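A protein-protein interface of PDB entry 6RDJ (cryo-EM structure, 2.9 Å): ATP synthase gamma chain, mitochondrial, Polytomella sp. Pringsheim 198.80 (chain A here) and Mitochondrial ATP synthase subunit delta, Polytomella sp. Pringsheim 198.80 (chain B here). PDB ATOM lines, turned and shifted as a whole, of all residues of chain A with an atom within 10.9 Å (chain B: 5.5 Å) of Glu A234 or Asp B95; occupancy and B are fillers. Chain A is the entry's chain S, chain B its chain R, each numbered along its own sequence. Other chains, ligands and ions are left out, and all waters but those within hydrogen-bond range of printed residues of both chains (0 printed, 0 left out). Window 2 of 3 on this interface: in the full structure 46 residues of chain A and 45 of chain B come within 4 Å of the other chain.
The backbone carbonyl oxygen (O) of Asp A232 sits at hydrogen-bond distance from the backbone NH (N) of Ile B108 (3.2 Å). N of Glu A234 lies within hydrogen-bond range of O of Ile B108 (3.2 Å). The side-chain carboxylate of Glu A234 lies close to the side-chain carboxylate of Asp B95 (3.1 Å).
The backbone NH of Val B94 sits at hydrogen-bond distance from the backbone carbonyl oxygen of Gln B110 (3.2 Å). The side-chain hydroxyl of Ser A236 is in hydrogen-bond range of a ring nitrogen (ND1) of His A237 (2.4 Å).
CD1 of Leu A88 touches CD1 of Ile B108, at 3.8 Å. Tyr A231 touches Thr B107 (CD1 to N, 3.6 Å). Thr B107 touches Asp A232 (CA to O, 3.3 Å). OE1 of Glu A234 touches CA of Gly B93 (3.6 Å). Val B94 touches Glu A234. CE1 of Phe B98 touches OE1 of Glu A234, 3.7 Å away. OE1 of Glu A234 touches CB of Ala B109, at 3.5 Å. Glu A234 touches Gln B110 (O to N, 3.8 Å). CG2 of Val B94 touches CA of Ala A235, 3.9 Å away. Leu A246 touches Ile B108 (CD2 to CG2, 3.8 Å).
Of chain A, only Glu A234 comes within 4 Å of Asp B95. Of chain A, only Glu A234 (3.6 Å) comes within 4 Å of Gly B93. Val B94 touches three residues of chain A. No residue of chain A comes within 4 Å of Gly B96. Ala B109 touches just one residue of chain A: Glu A234. Printed residues of chain B within 4 Å of Leu A88: Ile B108. Of the printed residues of chain B, Leu A246 touches Ile B108 (3.8 Å). Of the printed residues of chain A, Gln B110 touches Glu A234 (3.8 Å) and Ala A235 (3.8 Å). Leu A228 touches none of the printed residues of chain B. The nearest residue of chain B that does not touch Glu A234 is Gly B96 (4.3 Å).
Of the 18 printed residues of chain A, 8 touch a printed residue of chain B. Printed residues of chain A that touch a printed residue of chain B: Leu A88, Tyr A231, Asp A232, Ile A233, Glu A234, Ala A235, Ser A236 and Leu A246. Hydrophobic or aromatic side chains of chain A within 4 Å of the printed part of chain B: Leu A88, Tyr A231, Ile A233, Ala A235 and Leu A246. Of the 10 printed residues of chain B, 8 touch a printed residue of chain A. Printed residues of chain B that touch a printed residue of chain A: Gly B93, Val B94, Asp B95, Phe B98, Thr B107, Ile B108, Ala B109 and Gln B110. Hydrophobic or aromatic side chains of chain B within 4 Å of the printed part of chain A: Val B94, Phe B98, Ile B108 and Ala B109. Among the printed residues, 17 pairs touch across the chains. Among the printed residues, no Asp or Glu carboxylate lies within 4 Å of a Lys or Arg side-chain nitrogen of the other chain.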
ATOM      1  N   LEU A  88      17.670  13.911 -19.847  1.00  0.00           N
ATOM      2  CA  LEU A  88      18.960  14.583 -19.809  1.00  0.00           C
ATOM      3  C   LEU A  88      19.796  14.285 -21.042  1.00  0.00           C
ATOM      4  O   LEU A  88      20.422  15.189 -21.599  1.00  0.00           O
ATOM      5  CB  LEU A  88      19.722  14.161 -18.554  1.00  0.00           C
ATOM      6  CG  LEU A  88      21.126  14.719 -18.341  1.00  0.00           C
ATOM      7  CD1 LEU A  88      21.059  16.162 -17.918  1.00  0.00           C
ATOM      8  CD2 LEU A  88      21.859  13.899 -17.314  1.00  0.00           C
ATOM      9  N   LEU A 228      24.115  20.439 -23.781  1.00  0.00           N
ATOM     10  CA  LEU A 228      24.659  20.037 -22.498  1.00  0.00           C
ATOM     11  C   LEU A 228      25.388  21.165 -21.791  1.00  0.00           C
ATOM     12  O   LEU A 228      25.566  21.103 -20.572  1.00  0.00           O
ATOM     13  CB  LEU A 228      25.617  18.862 -22.687  1.00  0.00           C
ATOM     14  CG  LEU A 228      25.877  17.940 -21.504  1.00  0.00           C
ATOM     15  CD1 LEU A 228      24.701  17.025 -21.263  1.00  0.00           C
ATOM     16  CD2 LEU A 228      27.123  17.151 -21.794  1.00  0.00           C
ATOM     17  N   ALA A 230      24.231  24.001 -21.184  1.00  0.00           N
ATOM     18  CA  ALA A 230      23.327  24.730 -20.308  1.00  0.00           C
ATOM     19  C   ALA A 230      23.516  24.349 -18.848  1.00  0.00           C
ATOM     20  O   ALA A 230      23.164  25.135 -17.965  1.00  0.00           O
ATOM     21  CB  ALA A 230      21.880  24.483 -20.725  1.00  0.00           C
ATOM     22  N   TYR A 231      24.076  23.175 -18.579  1.00  0.00           N
ATOM     23  CA  TYR A 231      24.134  22.609 -17.240  1.00  0.00           C
ATOM     24  C   TYR A 231      25.426  22.995 -16.543  1.00  0.00           C
ATOM     25  O   TYR A 231      26.514  22.806 -17.090  1.00  0.00           O
ATOM     26  CB  TYR A 231      24.018  21.088 -17.294  1.00  0.00           C
ATOM     27  CG  TYR A 231      22.673  20.599 -17.749  1.00  0.00           C
ATOM     28  CD1 TYR A 231      21.657  20.365 -16.835  1.00  0.00           C
ATOM     29  CD2 TYR A 231      22.418  20.373 -19.085  1.00  0.00           C
ATOM     30  CE1 TYR A 231      20.430  19.923 -17.245  1.00  0.00           C
ATOM     31  CE2 TYR A 231      21.196  19.932 -19.504  1.00  0.00           C
ATOM     32  CZ  TYR A 231      20.206  19.708 -18.581  1.00  0.00           C
ATOM     33  OH  TYR A 231      18.983  19.262 -19.007  1.00  0.00           O
ATOM     34  N   ASP A 232      25.298  23.510 -15.331  1.00  0.00           N
ATOM     35  CA  ASP A 232      26.446  23.817 -14.499  1.00  0.00           C
ATOM     36  C   ASP A 232      26.939  22.535 -13.846  1.00  0.00           C
ATOM     37  O   ASP A 232      26.275  21.989 -12.966  1.00  0.00           O
ATOM     38  CB  ASP A 232      26.063  24.847 -13.438  1.00  0.00           C
ATOM     39  CG  ASP A 232      27.197  25.778 -13.091  1.00  0.00           C
ATOM     40  OD1 ASP A 232      27.200  26.310 -11.965  1.00  0.00           O
ATOM     41  OD2 ASP A 232      28.088  25.975 -13.940  1.00  0.00           O
ATOM     42  N   ILE A 233      28.107  22.070 -14.263  1.00  0.00           N
ATOM     43  CA  ILE A 233      28.631  20.803 -13.771  1.00  0.00           C
ATOM     44  C   ILE A 233      29.207  21.031 -12.385  1.00  0.00           C
ATOM     45  O   ILE A 233      30.028  21.928 -12.181  1.00  0.00           O
ATOM     46  CB  ILE A 233      29.688  20.238 -14.721  1.00  0.00           C
ATOM     47  CG1 ILE A 233      29.098  20.122 -16.113  1.00  0.00           C
ATOM     48  CG2 ILE A 233      30.167  18.896 -14.239  1.00  0.00           C
ATOM     49  CD1 ILE A 233      27.933  19.189 -16.198  1.00  0.00           C
ATOM     50  N   GLU A 234      28.767  20.227 -11.429  1.00  0.00           N
ATOM     51  CA  GLU A 234      29.152  20.381 -10.038  1.00  0.00           C
ATOM     52  C   GLU A 234      29.866  19.134  -9.544  1.00  0.00           C
ATOM     53  O   GLU A 234      29.649  18.675  -8.430  1.00  0.00           O
ATOM     54  CB  GLU A 234      27.926  20.692  -9.187  1.00  0.00           C
ATOM     55  CG  GLU A 234      28.166  21.581  -7.986  1.00  0.00           C
ATOM     56  CD  GLU A 234      28.240  20.809  -6.692  1.00  0.00           C
ATOM     57  OE1 GLU A 234      27.675  19.699  -6.622  1.00  0.00           O
ATOM     58  OE2 GLU A 234      28.846  21.321  -5.733  1.00  0.00           O
ATOM     59  N   ALA A 235      30.728  18.570 -10.369  1.00  0.00           N
ATOM     60  CA  ALA A 235      31.506  17.403  -9.993  1.00  0.00           C
ATOM     61  C   ALA A 235      32.900  17.833  -9.585  1.00  0.00           C
ATOM     62  O   ALA A 235      33.262  19.007  -9.660  1.00  0.00           O
ATOM     63  CB  ALA A 235      31.574  16.403 -11.141  1.00  0.00           C
ATOM     64  N   SER A 236      33.696  16.860  -9.151  1.00  0.00           N
ATOM     65  CA  SER A 236      35.070  17.155  -8.772  1.00  0.00           C
ATOM     66  C   SER A 236      35.930  17.389 -10.004  1.00  0.00           C
ATOM     67  O   SER A 236      36.509  18.464 -10.185  1.00  0.00           O
ATOM     68  CB  SER A 236      35.635  16.015  -7.932  1.00  0.00           C
ATOM     69  OG  SER A 236      36.010  14.931  -8.760  1.00  0.00           O
ATOM     70  N   HIS A 237      36.017  16.394 -10.862  1.00  0.00           N
ATOM     71  CA  HIS A 237      36.867  16.432 -12.038  1.00  0.00           C
ATOM     72  C   HIS A 237      36.062  16.932 -13.238  1.00  0.00           C
ATOM     73  O   HIS A 237      35.011  17.555 -13.080  1.00  0.00           O
ATOM     74  CB  HIS A 237      37.505  15.065 -12.235  1.00  0.00           C
ATOM     75  CG  HIS A 237      38.501  14.731 -11.174  1.00  0.00           C
ATOM     76  ND1 HIS A 237      38.143  14.522  -9.861  1.00  0.00           N
ATOM     77  CD2 HIS A 237      39.843  14.591 -11.225  1.00  0.00           C
ATOM     78  CE1 HIS A 237      39.223  14.257  -9.149  1.00  0.00           C
ATOM     79  NE2 HIS A 237      40.268  14.292  -9.953  1.00  0.00           N
ATOM     80  N   GLU A 238      36.576  16.713 -14.443  1.00  0.00           N
ATOM     81  CA  GLU A 238      36.052  17.337 -15.646  1.00  0.00           C
ATOM     82  C   GLU A 238      34.700  16.763 -16.050  1.00  0.00           C
ATOM     83  O   GLU A 238      34.205  15.788 -15.484  1.00  0.00           O
ATOM     84  CB  GLU A 238      37.049  17.183 -16.789  1.00  0.00           C
ATOM     85  CG  GLU A 238      38.224  18.105 -16.637  1.00  0.00           C
ATOM     86  CD  GLU A 238      37.821  19.551 -16.842  1.00  0.00           C
ATOM     87  OE1 GLU A 238      37.000  19.819 -17.744  1.00  0.00           O
ATOM     88  OE2 GLU A 238      38.283  20.416 -16.074  1.00  0.00           O
ATOM     89  N   ARG A 239      34.104  17.400 -17.060  1.00  0.00           N
ATOM     90  CA  ARG A 239      32.806  16.973 -17.559  1.00  0.00           C
ATOM     91  C   ARG A 239      32.895  15.659 -18.318  1.00  0.00           C
ATOM     92  O   ARG A 239      31.908  14.920 -18.386  1.00  0.00           O
ATOM     93  CB  ARG A 239      32.204  18.048 -18.451  1.00  0.00           C
ATOM     94  CG  ARG A 239      30.715  17.926 -18.591  1.00  0.00           C
ATOM     95  CD  ARG A 239      30.142  19.016 -19.438  1.00  0.00           C
ATOM     96  NE  ARG A 239      30.682  18.990 -20.782  1.00  0.00           N
ATOM     97  CZ  ARG A 239      30.228  19.756 -21.757  1.00  0.00           C
ATOM     98  NH1 ARG A 239      29.231  20.593 -21.523  1.00  0.00           N
ATOM     99  NH2 ARG A 239      30.767  19.687 -22.958  1.00  0.00           N
ATOM    100  N   SER A 240      34.056  15.354 -18.897  1.00  0.00           N
ATOM    101  CA  SER A 240      34.246  14.052 -19.519  1.00  0.00           C
ATOM    102  C   SER A 240      34.177  12.939 -18.486  1.00  0.00           C
ATOM    103  O   SER A 240      33.589  11.886 -18.739  1.00  0.00           O
ATOM    104  CB  SER A 240      35.576  14.014 -20.260  1.00  0.00           C
ATOM    105  OG  SER A 240      36.660  14.105 -19.355  1.00  0.00           O
ATOM    106  N   ASP A 241      34.722  13.176 -17.297  1.00  0.00           N
ATOM    107  CA  ASP A 241      34.637  12.198 -16.225  1.00  0.00           C
ATOM    108  C   ASP A 241      33.240  12.087 -15.642  1.00  0.00           C
ATOM    109  O   ASP A 241      32.819  10.978 -15.301  1.00  0.00           O
ATOM    110  CB  ASP A 241      35.629  12.546 -15.122  1.00  0.00           C
ATOM    111  CG  ASP A 241      37.032  12.737 -15.646  1.00  0.00           C
ATOM    112  OD1 ASP A 241      37.619  13.814 -15.416  1.00  0.00           O
ATOM    113  OD2 ASP A 241      37.553  11.808 -16.295  1.00  0.00           O
ATOM    114  N   VAL A 242      32.498  13.192 -15.547  1.00  0.00           N
ATOM    115  CA  VAL A 242      31.154  13.095 -14.995  1.00  0.00           C
ATOM    116  C   VAL A 242      30.217  12.448 -16.004  1.00  0.00           C
ATOM    117  O   VAL A 242      29.307  11.715 -15.626  1.00  0.00           O
ATOM    118  CB  VAL A 242      30.645  14.469 -14.500  1.00  0.00           C
ATOM    119  CG1 VAL A 242      30.112  15.352 -15.598  1.00  0.00           C
ATOM    120  CG2 VAL A 242      29.587  14.290 -13.487  1.00  0.00           C
ATOM    121  N   LEU A 243      30.476  12.616 -17.303  1.00  0.00           N
ATOM    122  CA  LEU A 243      29.690  11.905 -18.299  1.00  0.00           C
ATOM    123  C   LEU A 243      30.092  10.443 -18.386  1.00  0.00           C
ATOM    124  O   LEU A 243      29.250   9.589 -18.670  1.00  0.00           O
ATOM    125  CB  LEU A 243      29.834  12.581 -19.654  1.00  0.00           C
ATOM    126  CG  LEU A 243      28.667  13.446 -20.109  1.00  0.00           C
ATOM    127  CD1 LEU A 243      28.485  14.635 -19.218  1.00  0.00           C
ATOM    128  CD2 LEU A 243      28.929  13.899 -21.514  1.00  0.00           C
ATOM    129  N   ASP A 245      31.015   8.695 -15.790  1.00  0.00           N
ATOM    130  CA  ASP A 245      30.302   8.076 -14.678  1.00  0.00           C
ATOM    131  C   ASP A 245      28.805   7.999 -14.945  1.00  0.00           C
ATOM    132  O   ASP A 245      28.153   7.001 -14.610  1.00  0.00           O
ATOM    133  CB  ASP A 245      30.561   8.853 -13.393  1.00  0.00           C
ATOM    134  CG  ASP A 245      32.029   8.940 -13.055  1.00  0.00           C
ATOM    135  OD1 ASP A 245      32.370   9.562 -12.030  1.00  0.00           O
ATOM    136  OD2 ASP A 245      32.851   8.396 -13.819  1.00  0.00           O
ATOM    137  N   LEU A 246      28.260   9.030 -15.583  1.00  0.00           N
ATOM    138  CA  LEU A 246      26.828   9.155 -15.764  1.00  0.00           C
ATOM    139  C   LEU A 246      26.295   8.179 -16.797  1.00  0.00           C
ATOM    140  O   LEU A 246      25.175   7.698 -16.656  1.00  0.00           O
ATOM    141  CB  LEU A 246      26.520  10.590 -16.162  1.00  0.00           C
ATOM    142  CG  LEU A 246      25.171  11.194 -15.844  1.00  0.00           C
ATOM    143  CD1 LEU A 246      24.920  11.005 -14.396  1.00  0.00           C
ATOM    144  CD2 LEU A 246      25.241  12.657 -16.148  1.00  0.00           C
ATOM    145  N   GLY B  93      26.157  17.859  -2.475  1.00  0.00           N
ATOM    146  CA  GLY B  93      27.095  17.844  -3.579  1.00  0.00           C
ATOM    147  C   GLY B  93      28.522  17.609  -3.128  1.00  0.00           C
ATOM    148  O   GLY B  93      28.848  17.660  -1.944  1.00  0.00           O
ATOM    149  N   VAL B  94      29.390  17.313  -4.095  1.00  0.00           N
ATOM    150  CA  VAL B  94      30.754  16.945  -3.732  1.00  0.00           C
ATOM    151  C   VAL B  94      31.555  18.152  -3.275  1.00  0.00           C
ATOM    152  O   VAL B  94      32.506  18.008  -2.499  1.00  0.00           O
ATOM    153  CB  VAL B  94      31.456  16.222  -4.887  1.00  0.00           C
ATOM    154  CG1 VAL B  94      30.880  14.849  -5.069  1.00  0.00           C
ATOM    155  CG2 VAL B  94      31.293  17.001  -6.148  1.00  0.00           C
ATOM    156  N   ASP B  95      31.197  19.349  -3.729  1.00  0.00           N
ATOM    157  CA  ASP B  95      31.845  20.544  -3.220  1.00  0.00           C
ATOM    158  C   ASP B  95      31.283  20.930  -1.865  1.00  0.00           C
ATOM    159  O   ASP B  95      31.995  21.502  -1.034  1.00  0.00           O
ATOM    160  CB  ASP B  95      31.679  21.689  -4.211  1.00  0.00           C
ATOM    161  CG  ASP B  95      32.270  21.371  -5.567  1.00  0.00           C
ATOM    162  OD1 ASP B  95      31.742  21.871  -6.578  1.00  0.00           O
ATOM    163  OD2 ASP B  95      33.257  20.607  -5.624  1.00  0.00           O
ATOM    164  N   GLY B  96      30.030  20.604  -1.626  1.00  0.00           N
ATOM    165  CA  GLY B  96      29.381  20.893  -0.365  1.00  0.00           C
ATOM    166  C   GLY B  96      27.882  20.952  -0.560  1.00  0.00           C
ATOM    167  O   GLY B  96      27.376  20.877  -1.671  1.00  0.00           O
ATOM    168  N   TYR B  97      27.185  21.091   0.560  1.00  0.00           N
ATOM    169  CA  TYR B  97      25.729  21.090   0.553  1.00  0.00           C
ATOM    170  C   TYR B  97      25.211  22.341  -0.127  1.00  0.00           C
ATOM    171  O   TYR B  97      25.536  23.456   0.284  1.00  0.00           O
ATOM    172  CB  TYR B  97      25.195  21.010   1.978  1.00  0.00           C
ATOM    173  CG  TYR B  97      25.321  19.658   2.623  1.00  0.00           C
ATOM    174  CD1 TYR B  97      26.517  19.245   3.180  1.00  0.00           C
ATOM    175  CD2 TYR B  97      24.240  18.798   2.686  1.00  0.00           C
ATOM    176  CE1 TYR B  97      26.639  18.013   3.772  1.00  0.00           C
ATOM    177  CE2 TYR B  97      24.352  17.562   3.279  1.00  0.00           C
ATOM    178  CZ  TYR B  97      25.556  17.178   3.821  1.00  0.00           C
ATOM    179  OH  TYR B  97      25.686  15.948   4.419  1.00  0.00           O
ATOM    180  N   PHE B  98      24.417  22.172  -1.171  1.00  0.00           N
ATOM    181  CA  PHE B  98      23.762  23.300  -1.800  1.00  0.00           C
ATOM    182  C   PHE B  98      22.260  23.101  -1.728  1.00  0.00           C
ATOM    183  O   PHE B  98      21.772  22.004  -1.467  1.00  0.00           O
ATOM    184  CB  PHE B  98      24.224  23.496  -3.248  1.00  0.00           C
ATOM    185  CG  PHE B  98      23.883  22.367  -4.173  1.00  0.00           C
ATOM    186  CD1 PHE B  98      24.690  21.245  -4.257  1.00  0.00           C
ATOM    187  CD2 PHE B  98      22.785  22.452  -5.003  1.00  0.00           C
ATOM    188  CE1 PHE B  98      24.381  20.228  -5.111  1.00  0.00           C
ATOM    189  CE2 PHE B  98      22.480  21.437  -5.855  1.00  0.00           C
ATOM    190  CZ  PHE B  98      23.274  20.326  -5.905  1.00  0.00           C
ATOM    191  N   THR B 107      21.895  22.191 -13.781  1.00  0.00           N
ATOM    192  CA  THR B 107      22.975  21.628 -12.988  1.00  0.00           C
ATOM    193  C   THR B 107      23.003  20.123 -13.197  1.00  0.00           C
ATOM    194  O   THR B 107      21.950  19.498 -13.297  1.00  0.00           O
ATOM    195  CB  THR B 107      22.764  21.974 -11.505  1.00  0.00           C
ATOM    196  OG1 THR B 107      22.801  23.393 -11.338  1.00  0.00           O
ATOM    197  CG2 THR B 107      23.814  21.366 -10.616  1.00  0.00           C
ATOM    198  N   ILE B 108      24.199  19.557 -13.328  1.00  0.00           N
ATOM    199  CA  ILE B 108      24.421  18.123 -13.191  1.00  0.00           C
ATOM    200  C   ILE B 108      25.373  17.957 -12.017  1.00  0.00           C
ATOM    201  O   ILE B 108      26.596  17.981 -12.184  1.00  0.00           O
ATOM    202  CB  ILE B 108      24.988  17.493 -14.462  1.00  0.00           C
ATOM    203  CG1 ILE B 108      24.070  17.778 -15.638  1.00  0.00           C
ATOM    204  CG2 ILE B 108      25.121  16.006 -14.297  1.00  0.00           C
ATOM    205  CD1 ILE B 108      24.607  17.292 -16.947  1.00  0.00           C
ATOM    206  N   ALA B 109      24.828  17.794 -10.822  1.00  0.00           N
ATOM    207  CA  ALA B 109      25.623  17.752  -9.609  1.00  0.00           C
ATOM    208  C   ALA B 109      25.839  16.319  -9.176  1.00  0.00           C
ATOM    209  O   ALA B 109      24.877  15.580  -8.975  1.00  0.00           O
ATOM    210  CB  ALA B 109      24.948  18.526  -8.487  1.00  0.00           C
ATOM    211  N   GLN B 110      27.095  15.933  -9.025  1.00  0.00           N
ATOM    212  CA  GLN B 110      27.424  14.637  -8.467  1.00  0.00           C
ATOM    213  C   GLN B 110      27.344  14.740  -6.956  1.00  0.00           C
ATOM    214  O   GLN B 110      27.885  15.675  -6.368  1.00  0.00           O
ATOM    215  CB  GLN B 110      28.813  14.184  -8.896  1.00  0.00           C
ATOM    216  CG  GLN B 110      29.150  12.802  -8.400  1.00  0.00           C
ATOM    217  CD  GLN B 110      30.483  12.311  -8.887  1.00  0.00           C
ATOM    218  OE1 GLN B 110      31.051  12.853  -9.829  1.00  0.00           O
ATOM    219  NE2 GLN B 110      30.998  11.274  -8.244  1.00  0.00           N
